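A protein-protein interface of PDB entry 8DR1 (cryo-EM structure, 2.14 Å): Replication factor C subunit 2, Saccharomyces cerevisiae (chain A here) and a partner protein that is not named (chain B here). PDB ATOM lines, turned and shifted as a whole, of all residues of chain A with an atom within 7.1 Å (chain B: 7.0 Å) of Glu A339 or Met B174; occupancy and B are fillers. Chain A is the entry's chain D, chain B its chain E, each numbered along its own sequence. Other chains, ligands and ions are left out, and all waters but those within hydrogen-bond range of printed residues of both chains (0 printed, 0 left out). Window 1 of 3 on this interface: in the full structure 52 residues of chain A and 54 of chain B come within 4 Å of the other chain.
The side-chain hydroxyl of Ser B175 is in hydrogen-bond range of the backbone carbonyl oxygen of Thr A337, 3.0 Å away. N of Asn A338 is in hydrogen-bond range of OD2 of Asp B329 (2.8 Å). OG of Ser B173 is in hydrogen-bond range of OE2 of Glu A339.
The backbone NH (N) of Ala A297 sits at hydrogen-bond distance from the side-chain carboxylate (OE1) of Glu A339. OD1 of Asn A338 is in hydrogen-bond range of N of His A340 (3.1 Å). The side-chain amide oxygen (OD1) of Asn A338 lies within hydrogen-bond range of the backbone NH (N) of Ile A341, at 3.0 Å. O of Ile B188 lies within hydrogen-bond range of N of Tyr B42 (2.9 Å). ND2 of Asn B144 sits at hydrogen-bond distance from O of Ser B173, at 3.4 Å. The side-chain sulfur of Cys B171 lies within hydrogen-bond range of the backbone carbonyl oxygen of Ser B173, 3.3 Å away.
Among the printed residues, pairs that only touch across the chains: Gly A294 with Tyr B42 (3.3 Å), Leu A333 with Ser B175 (3.95 Å), Gly A336 with Ser B175 (3.2 Å), Gly A336 with Pro B176 (3.9 Å), Thr A337 with Asp B329 (3.0 Å), Glu A339 with Met B174 (3.9 Å), Glu A339 with Ser B175 (3.8 Å) and Gln A342 with Asp B329 (3.5 Å).
Of the printed residues of chain B, Leu A333 touches Ser B175. Glu A339 touches just these residues of chain B: Ser B173 (3.5 Å), Met B174 (3.9 Å) and Ser B175 (3.8 Å). Leu B40 touches none of the printed residues of chain A. Printed residues of chain A within 4 Å of Tyr B42: Gly A294 (3.3 Å). Of the printed residues of chain A, Met B174 touches Glu A339 (3.9 Å). Ile B178 touches none of the printed residues of chain A. Of the printed residues of chain A, Asp B329 touches Thr A337, Asn A338 and Gln A342. The nearest residue of chain B that does not touch Glu A339 is Asp B329 (5.8 Å). The nearest printed residue of chain B that does not touch Gln A342 is Ser B175 (7.6 Å).
Of the 17 printed residues of chain B, 6 touch a printed residue of chain A. Of the 19 printed residues of chain A, 7 touch a printed residue of chain B.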
ATOM      1  N   VAL A 287       7.219  10.146  43.461  1.00  0.00           N
ATOM      2  CA  VAL A 287       6.889  10.110  42.040  1.00  0.00           C
ATOM      3  C   VAL A 287       5.624   9.294  41.807  1.00  0.00           C
ATOM      4  O   VAL A 287       4.792   9.640  40.959  1.00  0.00           O
ATOM      5  CB  VAL A 287       8.079   9.564  41.231  1.00  0.00           C
ATOM      6  CG1 VAL A 287       7.675   9.312  39.787  1.00  0.00           C
ATOM      7  CG2 VAL A 287       9.247  10.532  41.294  1.00  0.00           C
ATOM      8  N   MET A 291       2.448  11.015  39.871  1.00  0.00           N
ATOM      9  CA  MET A 291       1.864  10.608  38.596  1.00  0.00           C
ATOM     10  C   MET A 291       0.345  10.508  38.651  1.00  0.00           C
ATOM     11  O   MET A 291      -0.303  10.550  37.601  1.00  0.00           O
ATOM     12  CB  MET A 291       2.443   9.268  38.136  1.00  0.00           C
ATOM     13  CG  MET A 291       3.943   9.272  37.903  1.00  0.00           C
ATOM     14  SD  MET A 291       4.440  10.463  36.646  1.00  0.00           S
ATOM     15  CE  MET A 291       3.920   9.612  35.160  1.00  0.00           C
ATOM     16  N   GLY A 294      -1.647  13.272  36.838  1.00  0.00           N
ATOM     17  CA  GLY A 294      -1.757  13.283  35.395  1.00  0.00           C
ATOM     18  C   GLY A 294      -0.899  14.302  34.682  1.00  0.00           C
ATOM     19  O   GLY A 294      -1.117  14.542  33.489  1.00  0.00           O
ATOM     20  N   TRP A 295       0.069  14.911  35.367  1.00  0.00           N
ATOM     21  CA  TRP A 295       0.935  15.889  34.725  1.00  0.00           C
ATOM     22  C   TRP A 295       1.672  15.259  33.549  1.00  0.00           C
ATOM     23  O   TRP A 295       2.112  14.108  33.614  1.00  0.00           O
ATOM     24  CB  TRP A 295       1.948  16.444  35.727  1.00  0.00           C
ATOM     25  CG  TRP A 295       1.335  17.094  36.923  1.00  0.00           C
ATOM     26  CD1 TRP A 295       1.384  16.650  38.211  1.00  0.00           C
ATOM     27  CD2 TRP A 295       0.582  18.311  36.947  1.00  0.00           C
ATOM     28  NE1 TRP A 295       0.709  17.514  39.036  1.00  0.00           N
ATOM     29  CE2 TRP A 295       0.205  18.542  38.285  1.00  0.00           C
ATOM     30  CE3 TRP A 295       0.189  19.227  35.968  1.00  0.00           C
ATOM     31  CZ2 TRP A 295      -0.546  19.649  38.667  1.00  0.00           C
ATOM     32  CZ3 TRP A 295      -0.555  20.326  36.350  1.00  0.00           C
ATOM     33  CH2 TRP A 295      -0.915  20.528  37.688  1.00  0.00           C
ATOM     34  N   SER A 296       1.803  16.023  32.468  1.00  0.00           N
ATOM     35  CA  SER A 296       2.559  15.559  31.312  1.00  0.00           C
ATOM     36  C   SER A 296       4.048  15.540  31.637  1.00  0.00           C
ATOM     37  O   SER A 296       4.591  16.510  32.174  1.00  0.00           O
ATOM     38  CB  SER A 296       2.290  16.461  30.109  1.00  0.00           C
ATOM     39  OG  SER A 296       3.348  16.387  29.171  1.00  0.00           O
ATOM     40  N   ALA A 297       4.713  14.431  31.302  1.00  0.00           N
ATOM     41  CA  ALA A 297       6.130  14.294  31.624  1.00  0.00           C
ATOM     42  C   ALA A 297       6.970  15.329  30.888  1.00  0.00           C
ATOM     43  O   ALA A 297       7.968  15.823  31.425  1.00  0.00           O
ATOM     44  CB  ALA A 297       6.610  12.883  31.290  1.00  0.00           C
ATOM     45  N   ALA A 298       6.594  15.660  29.651  1.00  0.00           N
ATOM     46  CA  ALA A 298       7.354  16.645  28.888  1.00  0.00           C
ATOM     47  C   ALA A 298       7.330  18.009  29.568  1.00  0.00           C
ATOM     48  O   ALA A 298       8.358  18.693  29.646  1.00  0.00           O
ATOM     49  CB  ALA A 298       6.802  16.746  27.467  1.00  0.00           C
ATOM     50  N   VAL A 300       6.904  18.576  32.773  1.00  0.00           N
ATOM     51  CA  VAL A 300       7.714  18.470  33.982  1.00  0.00           C
ATOM     52  C   VAL A 300       9.194  18.581  33.641  1.00  0.00           C
ATOM     53  O   VAL A 300       9.955  19.268  34.332  1.00  0.00           O
ATOM     54  CB  VAL A 300       7.406  17.153  34.720  1.00  0.00           C
ATOM     55  CG1 VAL A 300       8.296  17.010  35.946  1.00  0.00           C
ATOM     56  CG2 VAL A 300       5.938  17.088  35.116  1.00  0.00           C
ATOM     57  N   LEU A 333      11.430  10.347  25.645  1.00  0.00           N
ATOM     58  CA  LEU A 333      10.007  10.664  25.707  1.00  0.00           C
ATOM     59  C   LEU A 333       9.432  10.913  24.320  1.00  0.00           C
ATOM     60  O   LEU A 333       8.271  10.578  24.061  1.00  0.00           O
ATOM     61  CB  LEU A 333       9.776  11.885  26.598  1.00  0.00           C
ATOM     62  CG  LEU A 333       9.922  11.656  28.104  1.00  0.00           C
ATOM     63  CD1 LEU A 333       9.997  12.984  28.844  1.00  0.00           C
ATOM     64  CD2 LEU A 333       8.776  10.812  28.634  1.00  0.00           C
ATOM     65  N   GLY A 336       7.586   8.019  22.538  1.00  0.00           N
ATOM     66  CA  GLY A 336       6.341   7.459  23.025  1.00  0.00           C
ATOM     67  C   GLY A 336       6.542   6.443  24.132  1.00  0.00           C
ATOM     68  O   GLY A 336       5.921   5.376  24.122  1.00  0.00           O
ATOM     69  N   THR A 337       7.399   6.769  25.092  1.00  0.00           N
ATOM     70  CA  THR A 337       7.749   5.861  26.174  1.00  0.00           C
ATOM     71  C   THR A 337       6.850   6.086  27.390  1.00  0.00           C
ATOM     72  O   THR A 337       6.119   7.074  27.485  1.00  0.00           O
ATOM     73  CB  THR A 337       9.219   6.040  26.562  1.00  0.00           C
ATOM     74  OG1 THR A 337       9.539   7.435  26.613  1.00  0.00           O
ATOM     75  CG2 THR A 337      10.125   5.347  25.556  1.00  0.00           C
ATOM     76  N   ASN A 338       6.914   5.146  28.330  1.00  0.00           N
ATOM     77  CA  ASN A 338       6.132   5.242  29.557  1.00  0.00           C
ATOM     78  C   ASN A 338       6.641   6.406  30.402  1.00  0.00           C
ATOM     79  O   ASN A 338       7.814   6.436  30.788  1.00  0.00           O
ATOM     80  CB  ASN A 338       6.215   3.933  30.338  1.00  0.00           C
ATOM     81  CG  ASN A 338       5.432   3.975  31.636  1.00  0.00           C
ATOM     82  OD1 ASN A 338       5.935   4.426  32.664  1.00  0.00           O
ATOM     83  ND2 ASN A 338       4.192   3.507  31.592  1.00  0.00           N
ATOM     84  N   GLU A 339       5.754   7.358  30.697  1.00  0.00           N
ATOM     85  CA  GLU A 339       6.171   8.574  31.391  1.00  0.00           C
ATOM     86  C   GLU A 339       6.699   8.271  32.790  1.00  0.00           C
ATOM     87  O   GLU A 339       7.690   8.865  33.228  1.00  0.00           O
ATOM     88  CB  GLU A 339       5.002   9.556  31.459  1.00  0.00           C
ATOM     89  CG  GLU A 339       4.591  10.115  30.104  1.00  0.00           C
ATOM     90  CD  GLU A 339       3.681  11.324  30.214  1.00  0.00           C
ATOM     91  OE1 GLU A 339       3.525  11.860  31.332  1.00  0.00           O
ATOM     92  OE2 GLU A 339       3.119  11.741  29.179  1.00  0.00           O
ATOM     93  N   HIS A 340       6.044   7.356  33.507  1.00  0.00           N
ATOM     94  CA  HIS A 340       6.435   7.058  34.882  1.00  0.00           C
ATOM     95  C   HIS A 340       7.881   6.576  34.954  1.00  0.00           C
ATOM     96  O   HIS A 340       8.686   7.095  35.740  1.00  0.00           O
ATOM     97  CB  HIS A 340       5.482   6.009  35.460  1.00  0.00           C
ATOM     98  CG  HIS A 340       5.526   5.892  36.953  1.00  0.00           C
ATOM     99  ND1 HIS A 340       6.621   6.270  37.701  1.00  0.00           N
ATOM    100  CD2 HIS A 340       4.611   5.428  37.835  1.00  0.00           C
ATOM    101  CE1 HIS A 340       6.375   6.047  38.980  1.00  0.00           C
ATOM    102  NE2 HIS A 340       5.162   5.537  39.088  1.00  0.00           N
ATOM    103  N   ILE A 341       8.231   5.587  34.129  1.00  0.00           N
ATOM    104  CA  ILE A 341       9.571   5.008  34.173  1.00  0.00           C
ATOM    105  C   ILE A 341      10.615   6.057  33.810  1.00  0.00           C
ATOM    106  O   ILE A 341      11.638   6.203  34.491  1.00  0.00           O
ATOM    107  CB  ILE A 341       9.652   3.784  33.242  1.00  0.00           C
ATOM    108  CG1 ILE A 341       8.896   2.600  33.854  1.00  0.00           C
ATOM    109  CG2 ILE A 341      11.104   3.408  32.968  1.00  0.00           C
ATOM    110  CD1 ILE A 341       8.538   1.518  32.856  1.00  0.00           C
ATOM    111  N   GLN A 342      10.373   6.801  32.729  1.00  0.00           N
ATOM    112  CA  GLN A 342      11.346   7.795  32.287  1.00  0.00           C
ATOM    113  C   GLN A 342      11.550   8.873  33.345  1.00  0.00           C
ATOM    114  O   GLN A 342      12.689   9.260  33.636  1.00  0.00           O
ATOM    115  CB  GLN A 342      10.894   8.419  30.965  1.00  0.00           C
ATOM    116  CG  GLN A 342      10.684   7.420  29.832  1.00  0.00           C
ATOM    117  CD  GLN A 342      11.943   6.651  29.483  1.00  0.00           C
ATOM    118  OE1 GLN A 342      13.052   7.172  29.589  1.00  0.00           O
ATOM    119  NE2 GLN A 342      11.776   5.404  29.063  1.00  0.00           N
ATOM    120  N   LEU A 343      10.459   9.369  33.933  1.00  0.00           N
ATOM    121  CA  LEU A 343      10.575  10.419  34.939  1.00  0.00           C
ATOM    122  C   LEU A 343      11.305   9.920  36.179  1.00  0.00           C
ATOM    123  O   LEU A 343      12.159  10.628  36.729  1.00  0.00           O
ATOM    124  CB  LEU A 343       9.189  10.948  35.309  1.00  0.00           C
ATOM    125  CG  LEU A 343       9.158  12.059  36.363  1.00  0.00           C
ATOM    126  CD1 LEU A 343      10.008  13.244  35.927  1.00  0.00           C
ATOM    127  CD2 LEU A 343       7.729  12.498  36.641  1.00  0.00           C
ATOM    128  N   LEU A 344      10.979   8.710  36.642  1.00  0.00           N
ATOM    129  CA  LEU A 344      11.668   8.173  37.809  1.00  0.00           C
ATOM    130  C   LEU A 344      13.154   7.996  37.530  1.00  0.00           C
ATOM    131  O   LEU A 344      13.996   8.323  38.375  1.00  0.00           O
ATOM    132  CB  LEU A 344      11.039   6.845  38.231  1.00  0.00           C
ATOM    133  CG  LEU A 344      11.624   6.192  39.488  1.00  0.00           C
ATOM    134  CD1 LEU A 344      11.692   7.180  40.647  1.00  0.00           C
ATOM    135  CD2 LEU A 344      10.815   4.965  39.880  1.00  0.00           C
ATOM    136  N   ASN A 345      13.498   7.487  36.344  1.00  0.00           N
ATOM    137  CA  ASN A 345      14.905   7.327  35.991  1.00  0.00           C
ATOM    138  C   ASN A 345      15.619   8.673  35.984  1.00  0.00           C
ATOM    139  O   ASN A 345      16.726   8.804  36.520  1.00  0.00           O
ATOM    140  CB  ASN A 345      15.026   6.649  34.625  1.00  0.00           C
ATOM    141  CG  ASN A 345      16.467   6.423  34.211  1.00  0.00           C
ATOM    142  OD1 ASN A 345      17.275   5.909  34.984  1.00  0.00           O
ATOM    143  ND2 ASN A 345      16.798   6.815  32.987  1.00  0.00           N
ATOM    144  N   LEU B  40      -8.800  16.794  23.740  1.00  0.00           N
ATOM    145  CA  LEU B  40      -7.945  15.644  24.017  1.00  0.00           C
ATOM    146  C   LEU B  40      -7.834  15.496  25.529  1.00  0.00           C
ATOM    147  O   LEU B  40      -7.217  16.333  26.193  1.00  0.00           O
ATOM    148  CB  LEU B  40      -6.564  15.811  23.377  1.00  0.00           C
ATOM    149  CG  LEU B  40      -5.506  14.773  23.764  1.00  0.00           C
ATOM    150  CD1 LEU B  40      -6.043  13.357  23.623  1.00  0.00           C
ATOM    151  CD2 LEU B  40      -4.248  14.953  22.928  1.00  0.00           C
ATOM    152  N   LEU B  41      -8.430  14.436  26.067  1.00  0.00           N
ATOM    153  CA  LEU B  41      -8.457  14.185  27.503  1.00  0.00           C
ATOM    154  C   LEU B  41      -7.366  13.182  27.856  1.00  0.00           C
ATOM    155  O   LEU B  41      -7.370  12.052  27.351  1.00  0.00           O
ATOM    156  CB  LEU B  41      -9.822  13.656  27.943  1.00  0.00           C
ATOM    157  CG  LEU B  41     -10.935  14.685  28.143  1.00  0.00           C
ATOM    158  CD1 LEU B  41     -11.299  15.354  26.828  1.00  0.00           C
ATOM    159  CD2 LEU B  41     -12.154  14.027  28.772  1.00  0.00           C
ATOM    160  N   TYR B  42      -6.454  13.585  28.741  1.00  0.00           N
ATOM    161  CA  TYR B  42      -5.344  12.738  29.155  1.00  0.00           C
ATOM    162  C   TYR B  42      -5.305  12.634  30.673  1.00  0.00           C
ATOM    163  O   TYR B  42      -5.612  13.599  31.380  1.00  0.00           O
ATOM    164  CB  TYR B  42      -4.005  13.273  28.626  1.00  0.00           C
ATOM    165  CG  TYR B  42      -3.591  14.614  29.192  1.00  0.00           C
ATOM    166  CD1 TYR B  42      -4.087  15.798  28.663  1.00  0.00           C
ATOM    167  CD2 TYR B  42      -2.690  14.696  30.246  1.00  0.00           C
ATOM    168  CE1 TYR B  42      -3.705  17.025  29.174  1.00  0.00           C
ATOM    169  CE2 TYR B  42      -2.302  15.917  30.763  1.00  0.00           C
ATOM    170  CZ  TYR B  42      -2.812  17.079  30.224  1.00  0.00           C
ATOM    171  OH  TYR B  42      -2.428  18.297  30.734  1.00  0.00           O
ATOM    172  N   GLY B  43      -4.931  11.455  31.165  1.00  0.00           N
ATOM    173  CA  GLY B  43      -4.824  11.213  32.583  1.00  0.00           C
ATOM    174  C   GLY B  43      -4.647   9.741  32.901  1.00  0.00           C
ATOM    175  O   GLY B  43      -4.668   8.884  32.012  1.00  0.00           O
ATOM    176  N   ASN B 144      -3.729   7.247  21.708  1.00  0.00           N
ATOM    177  CA  ASN B 144      -2.277   7.134  21.773  1.00  0.00           C
ATOM    178  C   ASN B 144      -1.759   5.817  21.207  1.00  0.00           C
ATOM    179  O   ASN B 144      -0.541   5.626  21.149  1.00  0.00           O
ATOM    180  CB  ASN B 144      -1.802   7.307  23.219  1.00  0.00           C
ATOM    181  CG  ASN B 144      -2.324   6.224  24.144  1.00  0.00           C
ATOM    182  OD1 ASN B 144      -3.115   5.372  23.742  1.00  0.00           O
ATOM    183  ND2 ASN B 144      -1.881   6.256  25.394  1.00  0.00           N
ATOM    184  N   CYS B 171      -6.871   9.540  25.907  1.00  0.00           N
ATOM    185  CA  CYS B 171      -5.643   8.768  26.028  1.00  0.00           C
ATOM    186  C   CYS B 171      -5.208   8.724  27.485  1.00  0.00           C
ATOM    187  O   CYS B 171      -5.566   9.586  28.290  1.00  0.00           O
ATOM    188  CB  CYS B 171      -4.521   9.355  25.159  1.00  0.00           C
ATOM    189  SG  CYS B 171      -3.806  10.884  25.801  1.00  0.00           S
ATOM    190  N   ASP B 172      -4.431   7.694  27.816  1.00  0.00           N
ATOM    191  CA  ASP B 172      -3.836   7.574  29.139  1.00  0.00           C
ATOM    192  C   ASP B 172      -2.456   8.212  29.226  1.00  0.00           C
ATOM    193  O   ASP B 172      -1.879   8.257  30.317  1.00  0.00           O
ATOM    194  CB  ASP B 172      -3.752   6.096  29.549  1.00  0.00           C
ATOM    195  CG  ASP B 172      -2.848   5.279  28.638  1.00  0.00           C
ATOM    196  OD1 ASP B 172      -1.766   5.768  28.253  1.00  0.00           O
ATOM    197  OD2 ASP B 172      -3.225   4.135  28.307  1.00  0.00           O
ATOM    198  N   SER B 173      -1.919   8.700  28.110  1.00  0.00           N
ATOM    199  CA  SER B 173      -0.622   9.358  28.088  1.00  0.00           C
ATOM    200  C   SER B 173      -0.457  10.054  26.746  1.00  0.00           C
ATOM    201  O   SER B 173      -0.844   9.506  25.711  1.00  0.00           O
ATOM    202  CB  SER B 173       0.518   8.355  28.312  1.00  0.00           C
ATOM    203  OG  SER B 173       1.747   8.865  27.827  1.00  0.00           O
ATOM    204  N   MET B 174       0.118  11.253  26.772  1.00  0.00           N
ATOM    205  CA  MET B 174       0.297  12.050  25.567  1.00  0.00           C
ATOM    206  C   MET B 174       1.650  11.831  24.901  1.00  0.00           C
ATOM    207  O   MET B 174       1.896  12.400  23.833  1.00  0.00           O
ATOM    208  CB  MET B 174       0.128  13.537  25.896  1.00  0.00           C
ATOM    209  CG  MET B 174      -1.320  13.999  25.927  1.00  0.00           C
ATOM    210  SD  MET B 174      -1.473  15.793  25.865  1.00  0.00           S
ATOM    211  CE  MET B 174      -0.668  16.254  27.398  1.00  0.00           C
ATOM    212  N   SER B 175       2.526  11.022  25.494  1.00  0.00           N
ATOM    213  CA  SER B 175       3.849  10.821  24.909  1.00  0.00           C
ATOM    214  C   SER B 175       3.794  10.303  23.477  1.00  0.00           C
ATOM    215  O   SER B 175       4.584  10.789  22.647  1.00  0.00           O
ATOM    216  CB  SER B 175       4.674   9.883  25.802  1.00  0.00           C
ATOM    217  OG  SER B 175       4.543   8.530  25.406  1.00  0.00           O
ATOM    218  N   PRO B 176       2.933   9.347  23.114  1.00  0.00           N
ATOM    219  CA  PRO B 176       2.932   8.837  21.738  1.00  0.00           C
ATOM    220  C   PRO B 176       2.138   9.676  20.746  1.00  0.00           C
ATOM    221  O   PRO B 176       2.034   9.280  19.580  1.00  0.00           O
ATOM    222  CB  PRO B 176       2.305   7.434  21.889  1.00  0.00           C
ATOM    223  CG  PRO B 176       2.085   7.225  23.374  1.00  0.00           C
ATOM    224  CD  PRO B 176       2.003   8.588  23.962  1.00  0.00           C
ATOM    225  N   ILE B 177       1.578  10.811  21.156  1.00  0.00           N
ATOM    226  CA  ILE B 177       0.815  11.673  20.257  1.00  0.00           C
ATOM    227  C   ILE B 177       1.768  12.664  19.605  1.00  0.00           C
ATOM    228  O   ILE B 177       2.540  13.343  20.292  1.00  0.00           O
ATOM    229  CB  ILE B 177      -0.307  12.406  21.013  1.00  0.00           C
ATOM    230  CG1 ILE B 177      -1.224  11.410  21.733  1.00  0.00           C
ATOM    231  CG2 ILE B 177      -1.109  13.281  20.053  1.00  0.00           C
ATOM    232  CD1 ILE B 177      -2.121  10.607  20.814  1.00  0.00           C
ATOM    233  N   ILE B 178       1.713  12.754  18.273  1.00  0.00           N
ATOM    234  CA  ILE B 178       2.632  13.626  17.548  1.00  0.00           C
ATOM    235  C   ILE B 178       2.316  15.087  17.856  1.00  0.00           C
ATOM    236  O   ILE B 178       1.181  15.452  18.189  1.00  0.00           O
ATOM    237  CB  ILE B 178       2.575  13.351  16.034  1.00  0.00           C
ATOM    238  CG1 ILE B 178       1.188  13.677  15.468  1.00  0.00           C
ATOM    239  CG2 ILE B 178       2.945  11.903  15.748  1.00  0.00           C
ATOM    240  CD1 ILE B 178       1.065  13.435  13.975  1.00  0.00           C
ATOM    241  N   LYS B 182      -1.339  17.317  18.960  1.00  0.00           N
ATOM    242  CA  LYS B 182      -1.476  18.016  20.233  1.00  0.00           C
ATOM    243  C   LYS B 182      -1.701  19.505  20.019  1.00  0.00           C
ATOM    244  O   LYS B 182      -2.486  20.127  20.745  1.00  0.00           O
ATOM    245  CB  LYS B 182      -0.237  17.784  21.098  1.00  0.00           C
ATOM    246  CG  LYS B 182      -0.237  16.456  21.835  1.00  0.00           C
ATOM    247  CD  LYS B 182       1.165  16.049  22.271  1.00  0.00           C
ATOM    248  CE  LYS B 182       1.832  17.122  23.119  1.00  0.00           C
ATOM    249  NZ  LYS B 182       1.000  17.512  24.290  1.00  0.00           N
ATOM    250  N   LEU B 187      -6.148  20.519  25.318  1.00  0.00           N
ATOM    251  CA  LEU B 187      -5.687  19.464  26.209  1.00  0.00           C
ATOM    252  C   LEU B 187      -6.354  19.605  27.572  1.00  0.00           C
ATOM    253  O   LEU B 187      -6.342  20.687  28.166  1.00  0.00           O
ATOM    254  CB  LEU B 187      -4.165  19.514  26.356  1.00  0.00           C
ATOM    255  CG  LEU B 187      -3.373  19.691  25.057  1.00  0.00           C
ATOM    256  CD1 LEU B 187      -1.878  19.667  25.333  1.00  0.00           C
ATOM    257  CD2 LEU B 187      -3.748  18.627  24.036  1.00  0.00           C
ATOM    258  N   ILE B 188      -6.934  18.512  28.062  1.00  0.00           N
ATOM    259  CA  ILE B 188      -7.644  18.488  29.336  1.00  0.00           C
ATOM    260  C   ILE B 188      -7.006  17.424  30.218  1.00  0.00           C
ATOM    261  O   ILE B 188      -7.034  16.231  29.889  1.00  0.00           O
ATOM    262  CB  ILE B 188      -9.146  18.220  29.149  1.00  0.00           C
ATOM    263  CG1 ILE B 188      -9.771  19.294  28.253  1.00  0.00           C
ATOM    264  CG2 ILE B 188      -9.852  18.177  30.500  1.00  0.00           C
ATOM    265  CD1 ILE B 188     -11.175  18.968  27.786  1.00  0.00           C
ATOM    266  N   ASP B 329      12.108  -0.040  27.761  1.00  0.00           N
ATOM    267  CA  ASP B 329      10.829   0.549  27.387  1.00  0.00           C
ATOM    268  C   ASP B 329      10.954   1.299  26.067  1.00  0.00           C
ATOM    269  O   ASP B 329      10.090   1.174  25.185  1.00  0.00           O
ATOM    270  CB  ASP B 329      10.336   1.476  28.498  1.00  0.00           C
ATOM    271  CG  ASP B 329       9.052   2.192  28.135  1.00  0.00           C
ATOM    272  OD1 ASP B 329       8.014   1.517  27.979  1.00  0.00           O
ATOM    273  OD2 ASP B 329       9.077   3.432  28.014  1.00  0.00           O
